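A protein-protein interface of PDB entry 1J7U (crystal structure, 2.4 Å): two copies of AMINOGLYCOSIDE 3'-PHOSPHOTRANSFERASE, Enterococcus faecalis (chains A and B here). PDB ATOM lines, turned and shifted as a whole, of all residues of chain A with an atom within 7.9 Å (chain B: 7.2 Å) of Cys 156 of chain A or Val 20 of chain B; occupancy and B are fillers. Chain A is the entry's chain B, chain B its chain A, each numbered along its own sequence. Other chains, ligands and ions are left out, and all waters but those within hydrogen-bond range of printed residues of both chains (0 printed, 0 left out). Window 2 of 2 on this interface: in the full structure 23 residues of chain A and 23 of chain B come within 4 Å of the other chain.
No position is printed for both chains.
Of the 7 pairs that touch across the chains among the printed residues, none has its exchanged pair printed and touching as well.
The backbone NH of Val 20 of chain B is in hydrogen-bond range of the backbone carbonyl oxygen of Lys 33 of chain B.
Of the 14 printed residues of chain B, 4 touch a printed residue of chain A.
Hydrophobic or aromatic side chains of chain B that line the printed part of chain A: Tyr 32.
Among the printed residues, 7 pairs touch across the chains.
Among the printed residues, no Asp or Glu carboxylate lies within 4 Å of a Lys or Arg side-chain nitrogen of the other chain.
SG of Cys 19 of chain B forms a disulfide with SG of Cys 156 of chain A (2.0 Å).
SG of Cys 156 of chain A is in hydrogen-bond range of N of Val 20 of chain B (3.7 Å).
N of Lys 21 of chain B sits at hydrogen-bond distance from SG of Cys 156 of chain A (3.7 Å).
Val 20 of chain B touches just one residue of chain A: Cys 156 (3.7 Å).
Of the printed residues of chain A, Cys 19 of chain B touches Cys 156 (2.0 Å).
Of the printed residues of chain A, Tyr 32 of chain B touches Val 154, Asp 155, Cys 156 and Trp 159.
Of the printed residues of chain A, Lys 21 of chain B touches Cys 156 (3.7 Å).
Of the printed residues of chain B, Asp 155 of chain A touches Tyr 32 (3.8 Å).
Of the printed residues of chain B, Trp 159 of chain A touches Tyr 32.
Leu 34 of chain B touches none of the printed residues of chain A.
The nearest printed residue of chain B that does not touch Cys 156 of chain A is Lys 33 of chain B (6.0 Å).
Val 154 of chain A touches Tyr 32 of chain B (CB to OH, 3.6 Å).
O of Asp 155 of chain A touches OH of Tyr 32 of chain B, at 3.8 Å.
SG of Cys 156 of chain A touches CD2 of Tyr 32 of chain B, 3.8 Å away.
Tyr 32 of chain B touches Trp 159 of chain A (CE1 to CH2, 3.6 Å).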
ATOM      1  N   ASP A 153      -9.596  35.314 -30.370  1.00  0.00           N
ATOM      2  CA  ASP A 153      -9.455  34.340 -29.285  1.00  0.00           C
ATOM      3  C   ASP A 153      -8.274  33.388 -29.363  1.00  0.00           C
ATOM      4  O   ASP A 153      -8.012  32.768 -30.405  1.00  0.00           O
ATOM      5  CB  ASP A 153     -10.742  33.535 -29.073  1.00  0.00           C
ATOM      6  CG  ASP A 153     -10.691  32.675 -27.810  1.00  0.00           C
ATOM      7  OD1 ASP A 153     -11.080  33.173 -26.731  1.00  0.00           O
ATOM      8  OD2 ASP A 153     -10.244  31.511 -27.891  1.00  0.00           O
ATOM      9  N   VAL A 154      -7.605  33.260 -28.217  1.00  0.00           N
ATOM     10  CA  VAL A 154      -6.435  32.405 -28.045  1.00  0.00           C
ATOM     11  C   VAL A 154      -6.706  30.962 -28.446  1.00  0.00           C
ATOM     12  O   VAL A 154      -7.373  30.206 -27.727  1.00  0.00           O
ATOM     13  CB  VAL A 154      -5.905  32.459 -26.586  1.00  0.00           C
ATOM     14  N   ASP A 155      -6.193  30.601 -29.618  1.00  0.00           N
ATOM     15  CA  ASP A 155      -6.357  29.265 -30.165  1.00  0.00           C
ATOM     16  C   ASP A 155      -5.743  28.212 -29.244  1.00  0.00           C
ATOM     17  O   ASP A 155      -4.582  28.316 -28.852  1.00  0.00           O
ATOM     18  CB  ASP A 155      -5.722  29.192 -31.557  1.00  0.00           C
ATOM     19  N   CYS A 156      -6.557  27.236 -28.861  1.00  0.00           N
ATOM     20  CA  CYS A 156      -6.141  26.135 -27.992  1.00  0.00           C
ATOM     21  C   CYS A 156      -6.903  24.927 -28.517  1.00  0.00           C
ATOM     22  O   CYS A 156      -6.354  23.837 -28.651  1.00  0.00           O
ATOM     23  CB  CYS A 156      -6.508  26.447 -26.531  1.00  0.00           C
ATOM     24  SG  CYS A 156      -6.343  25.134 -25.264  1.00  0.00           S
ATOM     25  N   GLU A 157      -8.162  25.159 -28.874  1.00  0.00           N
ATOM     26  CA  GLU A 157      -9.022  24.123 -29.427  1.00  0.00           C
ATOM     27  C   GLU A 157      -8.792  24.063 -30.939  1.00  0.00           C
ATOM     28  O   GLU A 157      -8.801  22.984 -31.540  1.00  0.00           O
ATOM     29  CB  GLU A 157     -10.493  24.445 -29.131  1.00  0.00           C
ATOM     30  N   ASN A 158      -8.552  25.231 -31.534  1.00  0.00           N
ATOM     31  CA  ASN A 158      -8.317  25.351 -32.970  1.00  0.00           C
ATOM     32  C   ASN A 158      -6.985  24.760 -33.443  1.00  0.00           C
ATOM     33  O   ASN A 158      -6.619  24.905 -34.612  1.00  0.00           O
ATOM     34  CB  ASN A 158      -8.414  26.818 -33.399  1.00  0.00           C
ATOM     35  N   TRP A 159      -6.258  24.118 -32.530  1.00  0.00           N
ATOM     36  CA  TRP A 159      -4.975  23.493 -32.856  1.00  0.00           C
ATOM     37  C   TRP A 159      -5.144  21.990 -33.052  1.00  0.00           C
ATOM     38  O   TRP A 159      -4.282  21.328 -33.635  1.00  0.00           O
ATOM     39  CB  TRP A 159      -3.949  23.741 -31.747  1.00  0.00           C
ATOM     40  CG  TRP A 159      -3.474  25.155 -31.642  1.00  0.00           C
ATOM     41  CD1 TRP A 159      -3.568  26.127 -32.594  1.00  0.00           C
ATOM     42  CD2 TRP A 159      -2.815  25.752 -30.520  1.00  0.00           C
ATOM     43  NE1 TRP A 159      -3.007  27.295 -32.136  1.00  0.00           N
ATOM     44  CE2 TRP A 159      -2.536  27.092 -30.866  1.00  0.00           C
ATOM     45  CE3 TRP A 159      -2.432  25.285 -29.257  1.00  0.00           C
ATOM     46  CZ2 TRP A 159      -1.890  27.972 -29.992  1.00  0.00           C
ATOM     47  CZ3 TRP A 159      -1.790  26.161 -28.388  1.00  0.00           C
ATOM     48  CH2 TRP A 159      -1.526  27.489 -28.761  1.00  0.00           C
ATOM     49  N   GLU A 160      -6.255  21.459 -32.543  1.00  0.00           N
ATOM     50  CA  GLU A 160      -6.566  20.035 -32.641  1.00  0.00           C
ATOM     51  C   GLU A 160      -6.801  19.606 -34.089  1.00  0.00           C
ATOM     52  O   GLU A 160      -7.254  20.401 -34.916  1.00  0.00           O
ATOM     53  CB  GLU A 160      -7.797  19.710 -31.791  1.00  0.00           C
ATOM     54  N   ILE B  14       1.705  18.448 -31.608  1.00  0.00           N
ATOM     55  CA  ILE B  14       0.728  18.451 -30.520  1.00  0.00           C
ATOM     56  C   ILE B  14      -0.716  18.115 -30.896  1.00  0.00           C
ATOM     57  O   ILE B  14      -1.637  18.398 -30.126  1.00  0.00           O
ATOM     58  CB  ILE B  14       0.740  19.817 -29.787  1.00  0.00           C
ATOM     59  CG1 ILE B  14       0.396  20.942 -30.766  1.00  0.00           C
ATOM     60  CG2 ILE B  14       2.112  20.059 -29.142  1.00  0.00           C
ATOM     61  CD1 ILE B  14       0.134  22.270 -30.106  1.00  0.00           C
ATOM     62  N   TYR B  17      -2.734  15.653 -28.638  1.00  0.00           N
ATOM     63  CA  TYR B  17      -2.959  16.155 -27.292  1.00  0.00           C
ATOM     64  C   TYR B  17      -4.193  17.034 -27.212  1.00  0.00           C
ATOM     65  O   TYR B  17      -4.565  17.695 -28.182  1.00  0.00           O
ATOM     66  CB  TYR B  17      -1.731  16.929 -26.804  1.00  0.00           C
ATOM     67  CG  TYR B  17      -0.495  16.074 -26.644  1.00  0.00           C
ATOM     68  CD1 TYR B  17       0.365  15.842 -27.721  1.00  0.00           C
ATOM     69  CD2 TYR B  17      -0.186  15.488 -25.415  1.00  0.00           C
ATOM     70  CE1 TYR B  17       1.503  15.047 -27.577  1.00  0.00           C
ATOM     71  CE2 TYR B  17       0.944  14.691 -25.257  1.00  0.00           C
ATOM     72  CZ  TYR B  17       1.784  14.475 -26.339  1.00  0.00           C
ATOM     73  OH  TYR B  17       2.906  13.694 -26.177  1.00  0.00           O
ATOM     74  N   ARG B  18      -4.831  17.007 -26.048  1.00  0.00           N
ATOM     75  CA  ARG B  18      -6.025  17.797 -25.784  1.00  0.00           C
ATOM     76  C   ARG B  18      -5.594  19.057 -25.036  1.00  0.00           C
ATOM     77  O   ARG B  18      -5.159  18.987 -23.881  1.00  0.00           O
ATOM     78  CB  ARG B  18      -7.016  16.988 -24.938  1.00  0.00           C
ATOM     79  CG  ARG B  18      -8.380  17.641 -24.777  1.00  0.00           C
ATOM     80  N   CYS B  19      -5.705  20.201 -25.708  1.00  0.00           N
ATOM     81  CA  CYS B  19      -5.316  21.483 -25.130  1.00  0.00           C
ATOM     82  C   CYS B  19      -6.297  22.014 -24.095  1.00  0.00           C
ATOM     83  O   CYS B  19      -7.501  22.081 -24.339  1.00  0.00           O
ATOM     84  CB  CYS B  19      -5.119  22.523 -26.237  1.00  0.00           C
ATOM     85  SG  CYS B  19      -4.599  24.173 -25.660  1.00  0.00           S
ATOM     86  N   VAL B  20      -5.765  22.368 -22.930  1.00  0.00           N
ATOM     87  CA  VAL B  20      -6.549  22.932 -21.834  1.00  0.00           C
ATOM     88  C   VAL B  20      -5.762  24.097 -21.236  1.00  0.00           C
ATOM     89  O   VAL B  20      -4.763  23.902 -20.541  1.00  0.00           O
ATOM     90  CB  VAL B  20      -6.892  21.878 -20.736  1.00  0.00           C
ATOM     91  CG1 VAL B  20      -7.923  20.894 -21.259  1.00  0.00           C
ATOM     92  CG2 VAL B  20      -5.651  21.126 -20.292  1.00  0.00           C
ATOM     93  N   LYS B  21      -6.206  25.313 -21.544  1.00  0.00           N
ATOM     94  CA  LYS B  21      -5.555  26.531 -21.072  1.00  0.00           C
ATOM     95  C   LYS B  21      -5.484  26.635 -19.548  1.00  0.00           C
ATOM     96  O   LYS B  21      -6.451  26.333 -18.848  1.00  0.00           O
ATOM     97  CB  LYS B  21      -6.258  27.759 -21.656  1.00  0.00           C
ATOM     98  CG  LYS B  21      -5.611  29.091 -21.298  1.00  0.00           C
ATOM     99  CD  LYS B  21      -6.331  30.253 -21.975  1.00  0.00           C
ATOM    100  CE  LYS B  21      -5.821  31.604 -21.480  1.00  0.00           C
ATOM    101  NZ  LYS B  21      -4.377  31.822 -21.776  1.00  0.00           N
ATOM    102  N   ASP B  22      -4.321  27.059 -19.054  1.00  0.00           N
ATOM    103  CA  ASP B  22      -4.068  27.227 -17.622  1.00  0.00           C
ATOM    104  C   ASP B  22      -4.976  28.299 -17.008  1.00  0.00           C
ATOM    105  O   ASP B  22      -5.199  29.354 -17.606  1.00  0.00           O
ATOM    106  CB  ASP B  22      -2.595  27.589 -17.403  1.00  0.00           C
ATOM    107  CG  ASP B  22      -2.248  27.780 -15.942  1.00  0.00           C
ATOM    108  OD1 ASP B  22      -2.452  26.838 -15.143  1.00  0.00           O
ATOM    109  OD2 ASP B  22      -1.762  28.877 -15.597  1.00  0.00           O
ATOM    110  N   THR B  23      -5.474  28.022 -15.805  1.00  0.00           N
ATOM    111  CA  THR B  23      -6.377  28.928 -15.094  1.00  0.00           C
ATOM    112  C   THR B  23      -5.714  30.099 -14.358  1.00  0.00           C
ATOM    113  O   THR B  23      -6.335  31.150 -14.180  1.00  0.00           O
ATOM    114  CB  THR B  23      -7.280  28.146 -14.102  1.00  0.00           C
ATOM    115  N   VAL B  31      -0.195  29.758 -20.996  1.00  0.00           N
ATOM    116  CA  VAL B  31       0.237  28.421 -20.604  1.00  0.00           C
ATOM    117  C   VAL B  31      -0.842  27.412 -20.958  1.00  0.00           C
ATOM    118  O   VAL B  31      -2.008  27.594 -20.619  1.00  0.00           O
ATOM    119  CB  VAL B  31       0.529  28.326 -19.091  1.00  0.00           C
ATOM    120  CG1 VAL B  31       0.951  26.909 -18.727  1.00  0.00           C
ATOM    121  CG2 VAL B  31       1.614  29.319 -18.696  1.00  0.00           C
ATOM    122  N   TYR B  32      -0.445  26.342 -21.636  1.00  0.00           N
ATOM    123  CA  TYR B  32      -1.385  25.311 -22.049  1.00  0.00           C
ATOM    124  C   TYR B  32      -0.931  23.914 -21.650  1.00  0.00           C
ATOM    125  O   TYR B  32       0.183  23.504 -21.960  1.00  0.00           O
ATOM    126  CB  TYR B  32      -1.570  25.340 -23.570  1.00  0.00           C
ATOM    127  CG  TYR B  32      -1.981  26.679 -24.149  1.00  0.00           C
ATOM    128  CD1 TYR B  32      -1.048  27.512 -24.773  1.00  0.00           C
ATOM    129  CD2 TYR B  32      -3.310  27.096 -24.123  1.00  0.00           C
ATOM    130  CE1 TYR B  32      -1.434  28.721 -25.362  1.00  0.00           C
ATOM    131  CE2 TYR B  32      -3.701  28.296 -24.704  1.00  0.00           C
ATOM    132  CZ  TYR B  32      -2.758  29.101 -25.323  1.00  0.00           C
ATOM    133  OH  TYR B  32      -3.156  30.280 -25.914  1.00  0.00           O
ATOM    134  N   LYS B  33      -1.797  23.195 -20.945  1.00  0.00           N
ATOM    135  CA  LYS B  33      -1.527  21.815 -20.550  1.00  0.00           C
ATOM    136  C   LYS B  33      -2.056  20.979 -21.709  1.00  0.00           C
ATOM    137  O   LYS B  33      -3.228  21.087 -22.078  1.00  0.00           O
ATOM    138  CB  LYS B  33      -2.285  21.464 -19.265  1.00  0.00           C
ATOM    139  CG  LYS B  33      -2.090  20.033 -18.753  1.00  0.00           C
ATOM    140  CD  LYS B  33      -2.773  19.860 -17.394  1.00  0.00           C
ATOM    141  CE  LYS B  33      -2.465  18.517 -16.729  1.00  0.00           C
ATOM    142  NZ  LYS B  33      -3.185  17.373 -17.355  1.00  0.00           N
ATOM    143  N   LEU B  34      -1.174  20.203 -22.323  1.00  0.00           N
ATOM    144  CA  LEU B  34      -1.544  19.360 -23.451  1.00  0.00           C
ATOM    145  C   LEU B  34      -1.742  17.927 -22.965  1.00  0.00           C
ATOM    146  O   LEU B  34      -0.777  17.216 -22.691  1.00  0.00           O
ATOM    147  CB  LEU B  34      -0.462  19.448 -24.530  1.00  0.00           C
ATOM    148  CG  LEU B  34      -0.292  20.878 -25.064  1.00  0.00           C
ATOM    149  CD1 LEU B  34       1.016  21.050 -25.807  1.00  0.00           C
ATOM    150  CD2 LEU B  34      -1.467  21.239 -25.953  1.00  0.00           C
ATOM    151  N   VAL B  35      -3.007  17.533 -22.825  1.00  0.00           N
ATOM    152  CA  VAL B  35      -3.370  16.199 -22.340  1.00  0.00           C
ATOM    153  C   VAL B  35      -3.252  15.103 -23.395  1.00  0.00           C
ATOM    154  O   VAL B  35      -3.969  15.098 -24.396  1.00  0.00           O
ATOM    155  CB  VAL B  35      -4.810  16.170 -21.778  1.00  0.00           C
ATOM    156  CG1 VAL B  35      -5.068  14.856 -21.032  1.00  0.00           C
ATOM    157  CG2 VAL B  35      -5.040  17.358 -20.867  1.00  0.00           C
ATOM    158  N   TYR B  42       3.465  20.570 -21.829  1.00  0.00           N
ATOM    159  CA  TYR B  42       3.061  21.936 -21.556  1.00  0.00           C
ATOM    160  C   TYR B  42       3.635  22.854 -22.617  1.00  0.00           C
ATOM    161  O   TYR B  42       4.737  22.640 -23.104  1.00  0.00           O
ATOM    162  CB  TYR B  42       3.516  22.373 -20.163  1.00  0.00           C
ATOM    163  CG  TYR B  42       2.584  21.946 -19.054  1.00  0.00           C
ATOM    164  CD1 TYR B  42       2.735  20.714 -18.419  1.00  0.00           C
ATOM    165  CD2 TYR B  42       1.561  22.792 -18.617  1.00  0.00           C
ATOM    166  CE1 TYR B  42       1.891  20.334 -17.372  1.00  0.00           C
ATOM    167  CE2 TYR B  42       0.716  22.425 -17.573  1.00  0.00           C
ATOM    168  CZ  TYR B  42       0.888  21.198 -16.953  1.00  0.00           C
ATOM    169  OH  TYR B  42       0.072  20.860 -15.894  1.00  0.00           O
